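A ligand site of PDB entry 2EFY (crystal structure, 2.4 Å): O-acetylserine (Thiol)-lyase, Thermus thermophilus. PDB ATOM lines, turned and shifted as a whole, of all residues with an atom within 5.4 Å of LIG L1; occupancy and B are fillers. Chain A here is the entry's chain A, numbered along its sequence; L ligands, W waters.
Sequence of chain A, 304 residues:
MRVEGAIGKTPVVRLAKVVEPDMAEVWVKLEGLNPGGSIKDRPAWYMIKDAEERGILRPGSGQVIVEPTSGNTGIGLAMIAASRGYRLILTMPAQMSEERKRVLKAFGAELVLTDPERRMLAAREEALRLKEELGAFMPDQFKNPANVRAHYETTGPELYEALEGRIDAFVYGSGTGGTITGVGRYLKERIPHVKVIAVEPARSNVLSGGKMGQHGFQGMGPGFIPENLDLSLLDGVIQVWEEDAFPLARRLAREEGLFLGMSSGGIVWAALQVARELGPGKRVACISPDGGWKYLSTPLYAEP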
ATOM      1  N   SER A  38      29.653  19.168  -7.377  1.00  0.00           N
ATOM      2  CA  SER A  38      28.796  19.601  -6.289  1.00  0.00           C
ATOM      3  C   SER A  38      27.344  19.203  -6.464  1.00  0.00           C
ATOM      4  O   SER A  38      26.915  18.756  -7.532  1.00  0.00           O
ATOM      5  CB  SER A  38      28.861  21.118  -6.100  1.00  0.00           C
ATOM      6  OG  SER A  38      27.878  21.758  -6.905  1.00  0.00           O
ATOM      7  N   ILE A  39      26.592  19.377  -5.387  1.00  0.00           N
ATOM      8  CA  ILE A  39      25.173  19.056  -5.373  1.00  0.00           C
ATOM      9  C   ILE A  39      24.388  19.894  -6.391  1.00  0.00           C
ATOM     10  O   ILE A  39      23.273  19.538  -6.781  1.00  0.00           O
ATOM     11  CB  ILE A  39      24.627  19.327  -3.966  1.00  0.00           C
ATOM     12  CG1 ILE A  39      23.178  18.820  -3.862  1.00  0.00           C
ATOM     13  CG2 ILE A  39      24.702  20.823  -3.672  1.00  0.00           C
ATOM     14  CD1 ILE A  39      22.626  18.911  -2.468  1.00  0.00           C
ATOM     15  N   LYS A  40      24.966  21.011  -6.845  1.00  0.00           N
ATOM     16  CA  LYS A  40      24.257  21.860  -7.803  1.00  0.00           C
ATOM     17  C   LYS A  40      24.013  21.231  -9.177  1.00  0.00           C
ATOM     18  O   LYS A  40      23.200  21.734  -9.954  1.00  0.00           O
ATOM     19  CB  LYS A  40      24.977  23.203  -7.958  1.00  0.00           C
ATOM     20  CG  LYS A  40      24.883  24.117  -6.748  1.00  0.00           C
ATOM     21  CD  LYS A  40      23.427  24.352  -6.339  1.00  0.00           C
ATOM     22  CE  LYS A  40      23.297  25.582  -5.429  1.00  0.00           C
ATOM     23  NZ  LYS A  40      24.303  25.537  -4.347  1.00  0.00           N
ATOM     24  N   ASN A  72      28.640  27.176  -6.859  1.00  0.00           N
ATOM     25  CA  ASN A  72      28.468  25.913  -7.566  1.00  0.00           C
ATOM     26  C   ASN A  72      27.394  25.923  -8.651  1.00  0.00           C
ATOM     27  O   ASN A  72      27.503  25.173  -9.619  1.00  0.00           O
ATOM     28  CB  ASN A  72      28.175  24.777  -6.572  1.00  0.00           C
ATOM     29  CG  ASN A  72      29.363  24.460  -5.694  1.00  0.00           C
ATOM     30  OD1 ASN A  72      30.454  24.202  -6.191  1.00  0.00           O
ATOM     31  ND2 ASN A  72      29.155  24.476  -4.381  1.00  0.00           N
ATOM     32  N   THR A  73      26.363  26.750  -8.499  1.00  0.00           N
ATOM     33  CA  THR A  73      25.330  26.785  -9.527  1.00  0.00           C
ATOM     34  C   THR A  73      25.910  27.201 -10.881  1.00  0.00           C
ATOM     35  O   THR A  73      25.569  26.608 -11.908  1.00  0.00           O
ATOM     36  CB  THR A  73      24.167  27.741  -9.151  1.00  0.00           C
ATOM     37  OG1 THR A  73      23.538  27.267  -7.954  1.00  0.00           O
ATOM     38  CG2 THR A  73      23.127  27.785 -10.264  1.00  0.00           C
ATOM     39  N   ASN A 147      14.122  23.449  -8.868  1.00  0.00           N
ATOM     40  CA  ASN A 147      15.286  23.294  -8.007  1.00  0.00           C
ATOM     41  C   ASN A 147      14.879  22.246  -6.972  1.00  0.00           C
ATOM     42  O   ASN A 147      15.541  21.220  -6.809  1.00  0.00           O
ATOM     43  CB  ASN A 147      15.587  24.620  -7.307  1.00  0.00           C
ATOM     44  CG  ASN A 147      16.799  24.552  -6.382  1.00  0.00           C
ATOM     45  OD1 ASN A 147      17.075  23.519  -5.759  1.00  0.00           O
ATOM     46  ND2 ASN A 147      17.515  25.672  -6.272  1.00  0.00           N
ATOM     47  N   HIS A 151      15.608  17.519  -6.016  1.00  0.00           N
ATOM     48  CA  HIS A 151      15.915  16.823  -4.773  1.00  0.00           C
ATOM     49  C   HIS A 151      14.741  15.965  -4.323  1.00  0.00           C
ATOM     50  O   HIS A 151      14.906  14.988  -3.587  1.00  0.00           O
ATOM     51  CB  HIS A 151      16.272  17.841  -3.690  1.00  0.00           C
ATOM     52  CG  HIS A 151      17.406  18.740  -4.082  1.00  0.00           C
ATOM     53  ND1 HIS A 151      18.694  18.272  -4.255  1.00  0.00           N
ATOM     54  CD2 HIS A 151      17.442  20.053  -4.400  1.00  0.00           C
ATOM     55  CE1 HIS A 151      19.469  19.258  -4.657  1.00  0.00           C
ATOM     56  NE2 HIS A 151      18.729  20.357  -4.763  1.00  0.00           N
ATOM     57  N   TYR A 172      20.450  19.827   7.237  1.00  0.00           N
ATOM     58  CA  TYR A 172      21.038  20.456   6.069  1.00  0.00           C
ATOM     59  C   TYR A 172      21.204  21.972   6.196  1.00  0.00           C
ATOM     60  O   TYR A 172      20.356  22.653   6.768  1.00  0.00           O
ATOM     61  CB  TYR A 172      20.199  20.158   4.827  1.00  0.00           C
ATOM     62  CG  TYR A 172      20.886  20.544   3.534  1.00  0.00           C
ATOM     63  CD1 TYR A 172      21.953  19.796   3.039  1.00  0.00           C
ATOM     64  CD2 TYR A 172      20.505  21.691   2.829  1.00  0.00           C
ATOM     65  CE1 TYR A 172      22.617  20.169   1.893  1.00  0.00           C
ATOM     66  CE2 TYR A 172      21.176  22.084   1.674  1.00  0.00           C
ATOM     67  CZ  TYR A 172      22.228  21.313   1.211  1.00  0.00           C
ATOM     68  OH  TYR A 172      22.899  21.670   0.078  1.00  0.00           O
ATOM     69  N   GLY A 173      22.321  22.473   5.669  1.00  0.00           N
ATOM     70  CA  GLY A 173      22.602  23.904   5.690  1.00  0.00           C
ATOM     71  C   GLY A 173      21.972  24.518   4.452  1.00  0.00           C
ATOM     72  O   GLY A 173      22.531  24.462   3.358  1.00  0.00           O
ATOM     73  N   SER A 174      20.788  25.108   4.622  1.00  0.00           N
ATOM     74  CA  SER A 174      20.044  25.692   3.518  1.00  0.00           C
ATOM     75  C   SER A 174      20.663  26.881   2.791  1.00  0.00           C
ATOM     76  O   SER A 174      21.201  27.801   3.405  1.00  0.00           O
ATOM     77  CB  SER A 174      18.640  26.063   3.990  1.00  0.00           C
ATOM     78  OG  SER A 174      17.815  26.399   2.885  1.00  0.00           O
ATOM     79  N   GLY A 175      20.572  26.837   1.465  1.00  0.00           N
ATOM     80  CA  GLY A 175      21.078  27.907   0.621  1.00  0.00           C
ATOM     81  C   GLY A 175      19.910  28.424  -0.209  1.00  0.00           C
ATOM     82  O   GLY A 175      19.218  29.356   0.186  1.00  0.00           O
ATOM     83  N   THR A 176      19.674  27.804  -1.369  1.00  0.00           N
ATOM     84  CA  THR A 176      18.544  28.211  -2.192  1.00  0.00           C
ATOM     85  C   THR A 176      17.276  27.671  -1.531  1.00  0.00           C
ATOM     86  O   THR A 176      16.181  28.138  -1.815  1.00  0.00           O
ATOM     87  CB  THR A 176      18.606  27.645  -3.633  1.00  0.00           C
ATOM     88  OG1 THR A 176      18.543  26.225  -3.584  1.00  0.00           O
ATOM     89  CG2 THR A 176      19.888  28.089  -4.332  1.00  0.00           C
ATOM     90  N   GLY A 177      17.442  26.687  -0.652  1.00  0.00           N
ATOM     91  CA  GLY A 177      16.300  26.083   0.023  1.00  0.00           C
ATOM     92  C   GLY A 177      15.792  24.848  -0.698  1.00  0.00           C
ATOM     93  O   GLY A 177      14.951  24.102  -0.190  1.00  0.00           O
ATOM     94  N   GLY A 178      16.325  24.605  -1.888  1.00  0.00           N
ATOM     95  CA  GLY A 178      15.894  23.465  -2.686  1.00  0.00           C
ATOM     96  C   GLY A 178      16.155  22.085  -2.112  1.00  0.00           C
ATOM     97  O   GLY A 178      15.284  21.220  -2.159  1.00  0.00           O
ATOM     98  N   THR A 179      17.349  21.858  -1.586  1.00  0.00           N
ATOM     99  CA  THR A 179      17.688  20.552  -1.039  1.00  0.00           C
ATOM    100  C   THR A 179      16.842  20.171   0.181  1.00  0.00           C
ATOM    101  O   THR A 179      16.261  19.078   0.227  1.00  0.00           O
ATOM    102  CB  THR A 179      19.172  20.488  -0.620  1.00  0.00           C
ATOM    103  OG1 THR A 179      19.998  20.712  -1.773  1.00  0.00           O
ATOM    104  CG2 THR A 179      19.501  19.106  -0.022  1.00  0.00           C
ATOM    105  N   ILE A 180      16.782  21.064   1.156  1.00  0.00           N
ATOM    106  CA  ILE A 180      16.042  20.775   2.366  1.00  0.00           C
ATOM    107  C   ILE A 180      14.542  20.638   2.092  1.00  0.00           C
ATOM    108  O   ILE A 180      13.875  19.800   2.706  1.00  0.00           O
ATOM    109  CB  ILE A 180      16.319  21.838   3.470  1.00  0.00           C
ATOM    110  CG1 ILE A 180      16.043  21.225   4.842  1.00  0.00           C
ATOM    111  CG2 ILE A 180      15.476  23.083   3.239  1.00  0.00           C
ATOM    112  CD1 ILE A 180      16.620  22.033   6.009  1.00  0.00           C
ATOM    113  N   GLN A 218      30.556  29.277   2.555  1.00  0.00           N
ATOM    114  CA  GLN A 218      30.180  29.474   1.157  1.00  0.00           C
ATOM    115  C   GLN A 218      29.178  28.455   0.637  1.00  0.00           C
ATOM    116  O   GLN A 218      29.336  27.251   0.828  1.00  0.00           O
ATOM    117  CB  GLN A 218      31.423  29.452   0.262  1.00  0.00           C
ATOM    118  CG  GLN A 218      32.515  30.425   0.716  1.00  0.00           C
ATOM    119  CD  GLN A 218      33.735  30.422  -0.190  1.00  0.00           C
ATOM    120  OE1 GLN A 218      34.838  30.767   0.239  1.00  0.00           O
ATOM    121  NE2 GLN A 218      33.533  30.048  -1.448  1.00  0.00           N
ATOM    122  N   GLY A 219      28.125  28.956   0.002  1.00  0.00           N
ATOM    123  CA  GLY A 219      27.114  28.085  -0.545  1.00  0.00           C
ATOM    124  C   GLY A 219      25.809  28.103   0.232  1.00  0.00           C
ATOM    125  O   GLY A 219      24.758  27.850  -0.349  1.00  0.00           O
ATOM    126  N   MET A 220      25.869  28.415   1.514  1.00  0.00           N
ATOM    127  CA  MET A 220      24.647  28.446   2.327  1.00  0.00           C
ATOM    128  C   MET A 220      24.486  29.783   3.070  1.00  0.00           C
ATOM    129  O   MET A 220      25.375  30.637   3.056  1.00  0.00           O
ATOM    130  CB  MET A 220      24.666  27.288   3.331  1.00  0.00           C
ATOM    131  CG  MET A 220      25.863  27.340   4.281  1.00  0.00           C
ATOM    132  SD  MET A 220      25.838  26.107   5.608  1.00  0.00           S
ATOM    133  CE  MET A 220      24.764  26.904   6.793  1.00  0.00           C
ATOM    134  N   SER A 263      30.618  24.585   3.712  1.00  0.00           N
ATOM    135  CA  SER A 263      29.236  24.384   4.157  1.00  0.00           C
ATOM    136  C   SER A 263      29.117  23.020   4.840  1.00  0.00           C
ATOM    137  O   SER A 263      28.314  22.849   5.759  1.00  0.00           O
ATOM    138  CB  SER A 263      28.260  24.495   2.976  1.00  0.00           C
ATOM    139  OG  SER A 263      28.510  23.508   1.990  1.00  0.00           O
ATOM    140  N   ILE A 267      27.411  21.943   8.415  1.00  0.00           N
ATOM    141  CA  ILE A 267      26.313  21.004   8.357  1.00  0.00           C
ATOM    142  C   ILE A 267      26.575  19.765   9.204  1.00  0.00           C
ATOM    143  O   ILE A 267      25.742  19.366   9.999  1.00  0.00           O
ATOM    144  CB  ILE A 267      26.020  20.562   6.913  1.00  0.00           C
ATOM    145  CG1 ILE A 267      25.561  21.772   6.092  1.00  0.00           C
ATOM    146  CG2 ILE A 267      24.944  19.469   6.915  1.00  0.00           C
ATOM    147  CD1 ILE A 267      25.433  21.488   4.607  1.00  0.00           C
ATOM    148  N   PRO A 289      27.530  19.125   0.564  1.00  0.00           N
ATOM    149  CA  PRO A 289      27.338  19.799  -0.721  1.00  0.00           C
ATOM    150  C   PRO A 289      28.486  19.633  -1.722  1.00  0.00           C
ATOM    151  O   PRO A 289      28.244  19.432  -2.922  1.00  0.00           O
ATOM    152  CB  PRO A 289      27.121  21.240  -0.319  1.00  0.00           C
ATOM    153  CG  PRO A 289      26.374  21.089   0.985  1.00  0.00           C
ATOM    154  CD  PRO A 289      27.219  20.025   1.683  1.00  0.00           C
ATOM    155  N   ASP A 290      29.721  19.718  -1.252  1.00  0.00           N
ATOM    156  CA  ASP A 290      30.873  19.577  -2.140  1.00  0.00           C
ATOM    157  C   ASP A 290      32.161  19.291  -1.379  1.00  0.00           C
ATOM    158  O   ASP A 290      32.207  19.370  -0.160  1.00  0.00           O
ATOM    159  CB  ASP A 290      31.022  20.820  -3.029  1.00  0.00           C
ATOM    160  CG  ASP A 290      31.367  22.082  -2.245  1.00  0.00           C
ATOM    161  OD1 ASP A 290      31.389  23.168  -2.869  1.00  0.00           O
ATOM    162  OD2 ASP A 290      31.636  22.003  -1.021  1.00  0.00           O
ATOM    163  N   TYR A 295      38.336  25.291  -1.917  1.00  0.00           N
ATOM    164  CA  TYR A 295      38.505  26.162  -0.759  1.00  0.00           C
ATOM    165  C   TYR A 295      39.900  26.078  -0.160  1.00  0.00           C
ATOM    166  O   TYR A 295      40.107  26.410   1.011  1.00  0.00           O
ATOM    167  CB  TYR A 295      37.474  25.807   0.299  1.00  0.00           C
ATOM    168  CG  TYR A 295      36.070  25.695  -0.256  1.00  0.00           C
ATOM    169  CD1 TYR A 295      35.490  24.443  -0.498  1.00  0.00           C
ATOM    170  CD2 TYR A 295      35.338  26.835  -0.571  1.00  0.00           C
ATOM    171  CE1 TYR A 295      34.217  24.340  -1.040  1.00  0.00           C
ATOM    172  CE2 TYR A 295      34.068  26.745  -1.107  1.00  0.00           C
ATOM    173  CZ  TYR A 295      33.508  25.503  -1.345  1.00  0.00           C
ATOM    174  OH  TYR A 295      32.248  25.416  -1.889  1.00  0.00           O
HETATM  175  N1  LIG L   1      26.538  24.520   0.202  1.00  0.00           N
HETATM  176  C1  LIG L   1      27.077  24.657  -1.039  1.00  0.00           C
HETATM  177  C2  LIG L   1      28.653  24.624  -1.159  1.00  0.00           C
HETATM  178  C3  LIG L   1      26.248  24.826  -2.151  1.00  0.00           C
HETATM  179  O1  LIG L   1      26.785  24.980  -3.377  1.00  0.00           O
HETATM  180  C4  LIG L   1      24.863  24.852  -1.977  1.00  0.00           C
HETATM  181  C5  LIG L   1      23.949  25.015  -3.169  1.00  0.00           C
HETATM  182  C6  LIG L   1      24.333  24.703  -0.674  1.00  0.00           C
HETATM  183  C7  LIG L   1      25.187  24.531   0.376  1.00  0.00           C
HETATM  184  C8  LIG L   1      22.828  24.724  -0.308  1.00  0.00           C
HETATM  185  O2  LIG L   1      21.854  23.837  -0.940  1.00  0.00           O
HETATM  186  P1  LIG L   1      20.474  24.523  -1.447  1.00  0.00           P
HETATM  187  O3  LIG L   1      20.758  25.573  -2.446  1.00  0.00           O
HETATM  188  O4  LIG L   1      19.791  23.311  -2.209  1.00  0.00           O
HETATM  189  O5  LIG L   1      19.686  24.886  -0.269  1.00  0.00           O
HETATM  190  C1  LG2 L   2      24.966  29.459  -5.860  1.00  0.00           C
HETATM  191  O1  LG2 L   2      24.863  30.374  -6.578  1.00  0.00           O
HETATM  192  O2  LG2 L   2      25.808  28.456  -5.958  1.00  0.00           O
HETATM  193  C2  LG2 L   2      24.028  29.352  -4.630  1.00  0.00           C
HETATM  194  C3  LG2 L   2      24.522  30.322  -3.549  1.00  0.00           C
HETATM  195  C4  LG2 L   2      23.667  30.157  -2.420  1.00  0.00           C
HETATM  196  C5  LG2 L   2      22.836  30.568  -0.217  1.00  0.00           C
HETATM  197  C6  LG2 L   2      23.802  30.854  -1.307  1.00  0.00           C
HETATM  198  O3  LG2 L   2      24.690  31.694  -1.148  1.00  0.00           O
HETATM  199  O   HOH W   1      19.555  22.854  -4.918  1.00  0.00           O
HETATM  200  O   HOH W   2      31.221  25.440   0.878  1.00  0.00           O
HETATM  201  O   HOH W   3      18.059  23.651   1.527  1.00  0.00           O
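N of Thr 73 is in hydrogen-bond range of O2 of LG2 L2, 3.1 Å away. NZ of Lys 40 is in salt-bridge range of O2 of LG2 L2 (3.7 Å). An oxygen (O4) of LIG L1 sits at hydrogen-bond distance from the side-chain hydroxyl (OG1) of Thr 179, 2.6 Å away. The backbone NH of Thr 179 is in hydrogen-bond range of an oxygen (O4) of LIG L1, 2.9 Å away. O3 of LIG L1 sits at hydrogen-bond distance from OG1 of Thr 176, 2.6 Å away. N of Asn 72 sits at hydrogen-bond distance from O2 of LG2 L2, at 3.2 Å. O5 of LIG L1 sits at hydrogen-bond distance from N of Gly 175 (2.8 Å). An oxygen (O1) of LIG L1 lies within hydrogen-bond range of the side-chain amide nitrogen (ND2) of Asn 72. An oxygen (O2) of LIG L1 sits at hydrogen-bond distance from the side-chain hydroxyl (OH) of Tyr 172 (2.6 Å). An oxygen (O2) of LG2 L2 lies within hydrogen-bond range of the side-chain hydroxyl of Thr 73, 3.2 Å away. The side-chain hydroxyl of Ser 263 is in hydrogen-bond range of a nitrogen (N1) of LIG L1 (2.8 Å). N of Gly 177 is in hydrogen-bond range of O5 of LIG L1 (2.9 Å). The backbone NH (N) of Thr 176 is in hydrogen-bond range of an oxygen (O3) of LIG L1 (2.7 Å). C5 of LIG L1 is bonded to NZ of Lys 40.
Water W3 lies within hydrogen-bond range of O5 of LIG L1 (2.7 Å), N of Ile 180 (2.9 Å) and OG of Ser 174 (3.1 Å). Water W1 lies within hydrogen-bond range of a ring nitrogen (NE2) of His 151 (2.6 Å), the side-chain amide oxygen (OD1) of Asn 147 (2.7 Å) and an oxygen (O4) of LIG L1 (2.8 Å). Water W2 lies within hydrogen-bond range of O of Gln 218 (2.6 Å), OH of Tyr 295 (3.0 Å) and N of Ser 263 (3.0 Å).
A ring nitrogen (NE2) of His 151 sits at hydrogen-bond distance from the side-chain hydroxyl of Thr 179 (3.3 Å). OD1 of Asp 290 lies within hydrogen-bond range of OH of Tyr 295, at 2.6 Å. The backbone carbonyl oxygen (O) of Pro 289 lies within hydrogen-bond range of the backbone NH (N) of Ile 39 (3.0 Å). N of Lys 40 is in hydrogen-bond range of OG of Ser 38 (3.0 Å). OG1 of Thr 176 is in hydrogen-bond range of ND2 of Asn 147, 2.9 Å away. The side-chain carboxylate (OD1) of Asp 290 is in hydrogen-bond range of the side-chain amide nitrogen (ND2) of Asn 72 (3.0 Å). The backbone NH (N) of Gly 178 sits at hydrogen-bond distance from the side-chain hydroxyl (OG1) of Thr 176, at 3.2 Å.
O of Gly 173 touches C8 of LIG L1, at 3.7 Å. Ser 174 touches LIG L1 (C to O5, 3.8 Å). Gly 178 touches LIG L1 (N to O4, 3.7 Å). Gln 218 touches LIG L1 (O to C2, 3.4 Å). Gly 219 touches LIG L1. Pro 289 touches LIG L1 (CB to N1, 3.4 Å). Asp 290 touches LIG L1 (OD1 to C2, 3.5 Å). OH of Tyr 295 touches C2 of LIG L1 (3.8 Å). Hydrophobic or aromatic side chains within 4 Å of LIG L1: Tyr 172 and Pro 289. Within 4 Å of LIG L1: Lys 40, Asn 72, Tyr 172, Gly 173, Ser 174, Gly 175, Thr 176, Gly 177, Gly 178, Thr 179, Gln 218, Gly 219, Ser 263, Pro 289, Asp 290 and Tyr 295.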
